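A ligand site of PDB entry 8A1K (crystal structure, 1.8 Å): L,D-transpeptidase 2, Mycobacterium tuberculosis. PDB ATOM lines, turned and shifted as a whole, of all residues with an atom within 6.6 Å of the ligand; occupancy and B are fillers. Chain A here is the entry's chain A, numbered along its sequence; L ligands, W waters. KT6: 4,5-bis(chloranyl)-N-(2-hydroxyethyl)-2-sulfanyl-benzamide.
Met 250 touches the ligand.
Thr 267 touches the ligand (OG1 to CL13, 3.9 Å).
Val 269 touches the ligand.
Ser 278 touches the ligand (O to C19, 3.7 Å).
Val 280 touches the ligand.
Phe 281 touches the ligand (CD2 to S07, 3.8 Å).
His 283 touches the ligand (NE2 to C09, 3.3 Å).
CH2 of Trp 287 touches CL11 of the ligand, 3.7 Å away.
CA of Gly 300 touches O20 of the ligand, at 3.8 Å.
Hydrophobic or aromatic side chains within 4 Å of the ligand: Met 250, Tyr 265, Val 269, Phe 281, His 283, Trp 287 and His 299.
Within 4 Å of the ligand: Met 250, Tyr 265, Thr 267, Val 269, Ser 278, Gly 279, Val 280, Phe 281, His 283, Trp 287, His 299, Gly 300 and Cys 301.
The nearest printed residue that does not touch the ligand is Tyr 255 (4.7 Å).
The side-chain sulfur (SG) of Cys 301 sits at hydrogen-bond distance from the backbone NH (N) of Phe 281, at 3.5 Å.
The backbone carbonyl oxygen of Cys 301 sits at hydrogen-bond distance from the side-chain hydroxyl of Ser 298, at 2.8 Å.
The backbone NH of Gly 279 lies within hydrogen-bond range of the side-chain hydroxyl of Tyr 255 (2.9 Å).
The side-chain hydroxyl of Ser 276 sits at hydrogen-bond distance from the backbone NH of Gly 279, 3.2 Å away.
The backbone NH of Met 250 lies within hydrogen-bond range of the backbone carbonyl oxygen of Thr 267 (2.7 Å).
The backbone NH (N) of Val 280 is in hydrogen-bond range of the side-chain hydroxyl (OG) of Ser 276.
The backbone NH of Leu 302 is in hydrogen-bond range of the backbone carbonyl oxygen of Phe 281 (2.9 Å).
The backbone NH of Gly 300 lies within hydrogen-bond range of the side-chain hydroxyl of Ser 298 (2.9 Å).
Water W3 lies within hydrogen-bond range of O of Gly 279 (2.7 Å), N17 of the ligand (2.7 Å) and SD of Met 250 (3.4 Å).
Water W1 bridges NE2 of His 283 (2.9 Å) and ND2 of Asn 303 (2.9 Å).
A sulfur (S07) of the ligand is bonded to the side-chain sulfur of Cys 301, at 2.1 Å.
The side-chain hydroxyl (OH) of Tyr 265 sits at hydrogen-bond distance from a nitrogen (N17) of the ligand (3.1 Å).
N17 of the ligand sits close to O of Gly 279, 3.1 Å away.
The backbone carbonyl oxygen (O) of His 299 lies within hydrogen-bond range of an oxygen (O20) of the ligand.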
ATOM      1  N   THR A 232       7.837 -29.589  -3.062  1.00  0.00           N
ATOM      2  CA  THR A 232       8.308 -28.807  -1.920  1.00  0.00           C
ATOM      3  C   THR A 232       8.114 -29.641  -0.655  1.00  0.00           C
ATOM      4  O   THR A 232       7.264 -29.347   0.198  1.00  0.00           O
ATOM      5  CB  THR A 232       7.565 -27.471  -1.821  1.00  0.00           C
ATOM      6  OG1 THR A 232       6.189 -27.696  -1.615  1.00  0.00           O
ATOM      7  CG2 THR A 232       7.742 -26.645  -3.092  1.00  0.00           C
ATOM      8  N   PRO A 233       8.911 -30.679  -0.505  1.00  0.00           N
ATOM      9  CA  PRO A 233       8.646 -31.656   0.557  1.00  0.00           C
ATOM     10  C   PRO A 233       9.161 -31.216   1.919  1.00  0.00           C
ATOM     11  O   PRO A 233      10.034 -30.372   2.049  1.00  0.00           O
ATOM     12  CB  PRO A 233       9.400 -32.902   0.056  1.00  0.00           C
ATOM     13  CG  PRO A 233      10.558 -32.343  -0.691  1.00  0.00           C
ATOM     14  CD  PRO A 233      10.095 -31.036  -1.301  1.00  0.00           C
ATOM     15  N   MET A 250       2.891 -15.805   7.588  1.00  0.00           N
ATOM     16  CA  MET A 250       3.900 -16.594   6.927  1.00  0.00           C
ATOM     17  C   MET A 250       4.203 -15.940   5.591  1.00  0.00           C
ATOM     18  O   MET A 250       3.324 -15.830   4.762  1.00  0.00           O
ATOM     19  CB  MET A 250       3.416 -18.030   6.694  1.00  0.00           C
ATOM     20  CG  MET A 250       2.973 -18.756   7.962  1.00  0.00           C
ATOM     21  SD  MET A 250       4.414 -19.021   9.031  1.00  0.00           S
ATOM     22  CE  MET A 250       3.710 -20.219  10.176  1.00  0.00           C
ATOM     23  N   TYR A 255      12.654 -15.733   3.470  1.00  0.00           N
ATOM     24  CA  TYR A 255      13.642 -16.707   3.034  1.00  0.00           C
ATOM     25  C   TYR A 255      14.164 -16.458   1.629  1.00  0.00           C
ATOM     26  O   TYR A 255      14.673 -17.395   1.006  1.00  0.00           O
ATOM     27  CB  TYR A 255      13.033 -18.111   3.138  1.00  0.00           C
ATOM     28  CG  TYR A 255      12.699 -18.470   4.548  1.00  0.00           C
ATOM     29  CD1 TYR A 255      13.700 -18.839   5.433  1.00  0.00           C
ATOM     30  CD2 TYR A 255      11.398 -18.405   5.025  1.00  0.00           C
ATOM     31  CE1 TYR A 255      13.434 -19.117   6.717  1.00  0.00           C
ATOM     32  CE2 TYR A 255      11.109 -18.690   6.355  1.00  0.00           C
ATOM     33  CZ  TYR A 255      12.145 -19.041   7.175  1.00  0.00           C
ATOM     34  OH  TYR A 255      11.928 -19.374   8.509  1.00  0.00           O
ATOM     35  N   GLY A 264       6.310 -18.965  -3.844  1.00  0.00           N
ATOM     36  CA  GLY A 264       6.083 -17.935  -2.858  1.00  0.00           C
ATOM     37  C   GLY A 264       4.722 -17.997  -2.202  1.00  0.00           C
ATOM     38  O   GLY A 264       3.788 -18.621  -2.694  1.00  0.00           O
ATOM     39  N   TYR A 265       4.597 -17.278  -1.085  1.00  0.00           N
ATOM     40  CA  TYR A 265       3.356 -17.269  -0.337  1.00  0.00           C
ATOM     41  C   TYR A 265       3.383 -16.118   0.647  1.00  0.00           C
ATOM     42  O   TYR A 265       4.443 -15.613   1.022  1.00  0.00           O
ATOM     43  CB  TYR A 265       3.136 -18.600   0.415  1.00  0.00           C
ATOM     44  CG  TYR A 265       4.311 -18.963   1.260  1.00  0.00           C
ATOM     45  CD1 TYR A 265       4.485 -18.376   2.517  1.00  0.00           C
ATOM     46  CD2 TYR A 265       5.303 -19.797   0.762  1.00  0.00           C
ATOM     47  CE1 TYR A 265       5.644 -18.643   3.255  1.00  0.00           C
ATOM     48  CE2 TYR A 265       6.425 -20.089   1.509  1.00  0.00           C
ATOM     49  CZ  TYR A 265       6.585 -19.505   2.740  1.00  0.00           C
ATOM     50  OH  TYR A 265       7.724 -19.728   3.430  1.00  0.00           O
ATOM     51  N   ARG A 266       2.192 -15.679   1.036  1.00  0.00           N
ATOM     52  CA  ARG A 266       2.064 -14.728   2.138  1.00  0.00           C
ATOM     53  C   ARG A 266       0.665 -14.920   2.690  1.00  0.00           C
ATOM     54  O   ARG A 266      -0.316 -14.481   2.064  1.00  0.00           O
ATOM     55  CB  ARG A 266       2.307 -13.289   1.685  1.00  0.00           C
ATOM     56  CG  ARG A 266       2.187 -12.250   2.800  1.00  0.00           C
ATOM     57  CD  ARG A 266       2.634 -10.830   2.334  1.00  0.00           C
ATOM     58  NE  ARG A 266       1.981 -10.525   1.066  1.00  0.00           N
ATOM     59  CZ  ARG A 266       2.511  -9.834   0.100  1.00  0.00           C
ATOM     60  NH1 ARG A 266       3.751  -9.297   0.228  1.00  0.00           N
ATOM     61  NH2 ARG A 266       1.810  -9.638  -1.019  1.00  0.00           N
ATOM     62  N   THR A 267       0.563 -15.593   3.837  1.00  0.00           N
ATOM     63  CA  THR A 267      -0.715 -15.946   4.429  1.00  0.00           C
ATOM     64  C   THR A 267      -0.629 -15.835   5.950  1.00  0.00           C
ATOM     65  O   THR A 267       0.424 -16.090   6.556  1.00  0.00           O
ATOM     66  CB  THR A 267      -1.157 -17.382   4.072  1.00  0.00           C
ATOM     67  OG1 THR A 267      -0.653 -17.763   2.786  1.00  0.00           O
ATOM     68  CG2 THR A 267      -2.687 -17.460   4.031  1.00  0.00           C
ATOM     69  N   ASP A 268      -1.764 -15.505   6.564  1.00  0.00           N
ATOM     70  CA  ASP A 268      -1.890 -15.419   8.013  1.00  0.00           C
ATOM     71  C   ASP A 268      -2.458 -16.744   8.514  1.00  0.00           C
ATOM     72  O   ASP A 268      -3.438 -17.270   7.967  1.00  0.00           O
ATOM     73  CB  ASP A 268      -2.828 -14.238   8.351  1.00  0.00           C
ATOM     74  CG  ASP A 268      -2.823 -13.831   9.806  1.00  0.00           C
ATOM     75  OD1 ASP A 268      -2.158 -14.465  10.638  1.00  0.00           O
ATOM     76  OD2 ASP A 268      -3.537 -12.848  10.112  1.00  0.00           O
ATOM     77  N   VAL A 269      -1.817 -17.309   9.522  1.00  0.00           N
ATOM     78  CA  VAL A 269      -2.279 -18.589  10.059  1.00  0.00           C
ATOM     79  C   VAL A 269      -2.387 -18.508  11.571  1.00  0.00           C
ATOM     80  O   VAL A 269      -1.766 -17.670  12.231  1.00  0.00           O
ATOM     81  CB  VAL A 269      -1.359 -19.771   9.670  1.00  0.00           C
ATOM     82  CG1 VAL A 269      -1.135 -19.809   8.166  1.00  0.00           C
ATOM     83  CG2 VAL A 269      -0.024 -19.643  10.409  1.00  0.00           C
ATOM     84  N   SER A 276      11.586 -25.242  12.837  1.00  0.00           N
ATOM     85  CA  SER A 276      12.873 -25.027  12.193  1.00  0.00           C
ATOM     86  C   SER A 276      13.084 -23.554  11.853  1.00  0.00           C
ATOM     87  O   SER A 276      12.130 -22.792  11.625  1.00  0.00           O
ATOM     88  CB  SER A 276      13.026 -25.877  10.879  1.00  0.00           C
ATOM     89  OG  SER A 276      12.372 -25.248   9.769  1.00  0.00           O
ATOM     90  N   SER A 278      14.376 -22.700   9.177  1.00  0.00           N
ATOM     91  CA  SER A 278      14.032 -22.623   7.774  1.00  0.00           C
ATOM     92  C   SER A 278      12.531 -22.367   7.564  1.00  0.00           C
ATOM     93  O   SER A 278      12.107 -22.253   6.418  1.00  0.00           O
ATOM     94  CB  SER A 278      14.467 -23.879   7.037  1.00  0.00           C
ATOM     95  OG  SER A 278      13.737 -25.015   7.466  1.00  0.00           O
ATOM     96  N   GLY A 279      11.759 -22.270   8.653  1.00  0.00           N
ATOM     97  CA  GLY A 279      10.376 -21.837   8.584  1.00  0.00           C
ATOM     98  C   GLY A 279       9.340 -22.929   8.644  1.00  0.00           C
ATOM     99  O   GLY A 279       8.143 -22.652   8.336  1.00  0.00           O
ATOM    100  N   VAL A 280       9.712 -24.147   9.019  1.00  0.00           N
ATOM    101  CA  VAL A 280       8.731 -25.220   9.206  1.00  0.00           C
ATOM    102  C   VAL A 280       8.018 -24.977  10.526  1.00  0.00           C
ATOM    103  O   VAL A 280       8.647 -24.774  11.567  1.00  0.00           O
ATOM    104  CB  VAL A 280       9.389 -26.608   9.167  1.00  0.00           C
ATOM    105  CG1 VAL A 280       8.343 -27.681   9.371  1.00  0.00           C
ATOM    106  CG2 VAL A 280      10.110 -26.817   7.802  1.00  0.00           C
ATOM    107  N   PHE A 281       6.693 -25.035  10.477  1.00  0.00           N
ATOM    108  CA  PHE A 281       5.817 -24.932  11.621  1.00  0.00           C
ATOM    109  C   PHE A 281       4.785 -26.057  11.578  1.00  0.00           C
ATOM    110  O   PHE A 281       4.461 -26.590  10.513  1.00  0.00           O
ATOM    111  CB  PHE A 281       4.983 -23.625  11.612  1.00  0.00           C
ATOM    112  CG  PHE A 281       5.738 -22.380  11.907  1.00  0.00           C
ATOM    113  CD1 PHE A 281       5.550 -21.706  13.113  1.00  0.00           C
ATOM    114  CD2 PHE A 281       6.627 -21.850  10.979  1.00  0.00           C
ATOM    115  CE1 PHE A 281       6.248 -20.539  13.386  1.00  0.00           C
ATOM    116  CE2 PHE A 281       7.310 -20.692  11.279  1.00  0.00           C
ATOM    117  CZ  PHE A 281       7.111 -20.052  12.465  1.00  0.00           C
ATOM    118  N   VAL A 282       4.221 -26.345  12.742  1.00  0.00           N
ATOM    119  CA  VAL A 282       2.923 -26.995  12.869  1.00  0.00           C
ATOM    120  C   VAL A 282       1.906 -25.878  13.011  1.00  0.00           C
ATOM    121  O   VAL A 282       2.114 -24.993  13.845  1.00  0.00           O
ATOM    122  CB  VAL A 282       2.883 -27.921  14.102  1.00  0.00           C
ATOM    123  CG1 VAL A 282       1.436 -28.496  14.309  1.00  0.00           C
ATOM    124  CG2 VAL A 282       3.928 -29.069  13.965  1.00  0.00           C
ATOM    125  N   HIS A 283       0.848 -25.878  12.190  1.00  0.00           N
ATOM    126  CA  HIS A 283      -0.099 -24.787  12.265  1.00  0.00           C
ATOM    127  C   HIS A 283      -1.473 -25.198  11.792  1.00  0.00           C
ATOM    128  O   HIS A 283      -1.640 -26.246  11.140  1.00  0.00           O
ATOM    129  CB  HIS A 283       0.357 -23.537  11.469  1.00  0.00           C
ATOM    130  CG  HIS A 283       0.392 -23.727   9.965  1.00  0.00           C
ATOM    131  ND1 HIS A 283      -0.736 -23.635   9.169  1.00  0.00           N
ATOM    132  CD2 HIS A 283       1.412 -24.065   9.133  1.00  0.00           C
ATOM    133  CE1 HIS A 283      -0.404 -23.873   7.922  1.00  0.00           C
ATOM    134  NE2 HIS A 283       0.886 -24.170   7.868  1.00  0.00           N
ATOM    135  N   SER A 284      -2.441 -24.366  12.148  1.00  0.00           N
ATOM    136  CA  SER A 284      -3.814 -24.583  11.712  1.00  0.00           C
ATOM    137  C   SER A 284      -3.922 -24.357  10.208  1.00  0.00           C
ATOM    138  O   SER A 284      -3.458 -23.347   9.679  1.00  0.00           O
ATOM    139  CB  SER A 284      -4.734 -23.615  12.459  1.00  0.00           C
ATOM    140  OG  SER A 284      -6.074 -23.649  11.944  1.00  0.00           O
ATOM    141  N   TRP A 287      -7.918 -25.022   5.260  1.00  0.00           N
ATOM    142  CA  TRP A 287      -8.074 -25.257   3.837  1.00  0.00           C
ATOM    143  C   TRP A 287      -7.589 -26.618   3.376  1.00  0.00           C
ATOM    144  O   TRP A 287      -7.860 -26.983   2.231  1.00  0.00           O
ATOM    145  CB  TRP A 287      -7.334 -24.158   3.037  1.00  0.00           C
ATOM    146  CG  TRP A 287      -5.859 -24.210   3.315  1.00  0.00           C
ATOM    147  CD1 TRP A 287      -4.943 -24.996   2.681  1.00  0.00           C
ATOM    148  CD2 TRP A 287      -5.128 -23.474   4.318  1.00  0.00           C
ATOM    149  NE1 TRP A 287      -3.685 -24.791   3.235  1.00  0.00           N
ATOM    150  CE2 TRP A 287      -3.789 -23.856   4.219  1.00  0.00           C
ATOM    151  CE3 TRP A 287      -5.490 -22.525   5.272  1.00  0.00           C
ATOM    152  CZ2 TRP A 287      -2.795 -23.332   5.056  1.00  0.00           C
ATOM    153  CZ3 TRP A 287      -4.479 -21.992   6.114  1.00  0.00           C
ATOM    154  CH2 TRP A 287      -3.179 -22.391   5.980  1.00  0.00           C
ATOM    155  N   SER A 298       1.303 -29.057   1.140  1.00  0.00           N
ATOM    156  CA  SER A 298       1.845 -27.796   1.630  1.00  0.00           C
ATOM    157  C   SER A 298       3.183 -27.494   0.972  1.00  0.00           C
ATOM    158  O   SER A 298       3.643 -28.207   0.088  1.00  0.00           O
ATOM    159  CB  SER A 298       2.006 -27.824   3.147  1.00  0.00           C
ATOM    160  OG  SER A 298       3.232 -28.477   3.523  1.00  0.00           O
ATOM    161  N   HIS A 299       3.798 -26.387   1.383  1.00  0.00           N
ATOM    162  CA  HIS A 299       5.120 -25.987   0.944  1.00  0.00           C
ATOM    163  C   HIS A 299       6.227 -26.557   1.836  1.00  0.00           C
ATOM    164  O   HIS A 299       7.405 -26.203   1.661  1.00  0.00           O
ATOM    165  CB  HIS A 299       5.252 -24.439   0.941  1.00  0.00           C
ATOM    166  CG  HIS A 299       4.398 -23.763  -0.071  1.00  0.00           C
ATOM    167  ND1 HIS A 299       3.082 -23.433   0.153  1.00  0.00           N
ATOM    168  CD2 HIS A 299       4.679 -23.332  -1.328  1.00  0.00           C
ATOM    169  CE1 HIS A 299       2.582 -22.865  -0.929  1.00  0.00           C
ATOM    170  NE2 HIS A 299       3.540 -22.763  -1.830  1.00  0.00           N
ATOM    171  N   GLY A 300       5.860 -27.380   2.811  1.00  0.00           N
ATOM    172  CA  GLY A 300       6.801 -27.959   3.758  1.00  0.00           C
ATOM    173  C   GLY A 300       6.316 -28.019   5.171  1.00  0.00           C
ATOM    174  O   GLY A 300       6.811 -28.804   5.978  1.00  0.00           O
ATOM    175  N   CYS A 301       5.366 -27.148   5.517  1.00  0.00           N
ATOM    176  CA  CYS A 301       4.865 -27.157   6.895  1.00  0.00           C
ATOM    177  C   CYS A 301       3.885 -28.304   7.202  1.00  0.00           C
ATOM    178  O   CYS A 301       3.335 -28.893   6.305  1.00  0.00           O
ATOM    179  CB  CYS A 301       4.227 -25.804   7.187  1.00  0.00           C
ATOM    180  SG  CYS A 301       5.572 -24.548   7.250  1.00  0.00           S
ATOM    181  N   LEU A 302       3.693 -28.586   8.484  1.00  0.00           N
ATOM    182  CA  LEU A 302       2.832 -29.646   8.969  1.00  0.00           C
ATOM    183  C   LEU A 302       1.459 -29.034   9.193  1.00  0.00           C
ATOM    184  O   LEU A 302       1.183 -28.465  10.260  1.00  0.00           O
ATOM    185  CB  LEU A 302       3.387 -30.276  10.245  1.00  0.00           C
ATOM    186  CG  LEU A 302       4.511 -31.295  10.013  1.00  0.00           C
ATOM    187  CD1 LEU A 302       5.692 -30.700   9.314  1.00  0.00           C
ATOM    188  CD2 LEU A 302       4.894 -31.963  11.367  1.00  0.00           C
ATOM    189  N   ASN A 303       0.579 -29.209   8.188  1.00  0.00           N
ATOM    190  CA  ASN A 303      -0.811 -28.773   8.279  1.00  0.00           C
ATOM    191  C   ASN A 303      -1.594 -29.706   9.190  1.00  0.00           C
ATOM    192  O   ASN A 303      -1.589 -30.914   8.969  1.00  0.00           O
ATOM    193  CB  ASN A 303      -1.444 -28.783   6.892  1.00  0.00           C
ATOM    194  CG  ASN A 303      -0.997 -27.666   5.982  1.00  0.00           C
ATOM    195  OD1 ASN A 303      -1.709 -27.368   5.017  1.00  0.00           O
ATOM    196  ND2 ASN A 303       0.179 -27.098   6.221  1.00  0.00           N
HETATM  197  C10 KT6 L   1       1.936 -21.489   5.183  1.00  0.00           C
HETATM  198  C15 KT6 L   1       4.595 -22.104   4.978  1.00  0.00           C
HETATM  199  C08 KT6 L   1       3.960 -22.173   6.212  1.00  0.00           C
HETATM  200  C09 KT6 L   1       2.627 -21.853   6.322  1.00  0.00           C
HETATM  201  C12 KT6 L   1       2.547 -21.427   3.961  1.00  0.00           C
HETATM  202  C14 KT6 L   1       3.888 -21.712   3.839  1.00  0.00           C
HETATM  203  C16 KT6 L   1       6.034 -22.455   4.698  1.00  0.00           C
HETATM  204  C18 KT6 L   1       8.470 -22.345   5.025  1.00  0.00           C
HETATM  205  C19 KT6 L   1       8.839 -23.748   5.502  1.00  0.00           C
HETATM  206  N17 KT6 L   1       7.131 -21.953   5.437  1.00  0.00           N
HETATM  207  O20 KT6 L   1       8.550 -24.623   4.426  1.00  0.00           O
HETATM  208  O21 KT6 L   1       6.192 -23.273   3.827  1.00  0.00           O
HETATM  209  S07 KT6 L   1       4.774 -22.659   7.758  1.00  0.00           S
HETATM  210 CL11 KT6 L   1       0.218 -21.155   5.331  1.00  0.00          CL
HETATM  211 CL13 KT6 L   1       1.646 -20.955   2.525  1.00  0.00          CL
HETATM  212  O   HOH W   1       1.350 -24.699   5.096  1.00  0.00           O
HETATM  213  O   HOH W   2       3.863 -25.047   4.052  1.00  0.00           O
HETATM  214  O   HOH W   3       7.182 -20.291   7.574  1.00  0.00           O
HETATM  215  O   HOH W   4      -0.774 -19.973   0.213  1.00  0.00           O
HETATM  216  O   HOH W   5      10.305 -26.819   4.102  1.00  0.00           O
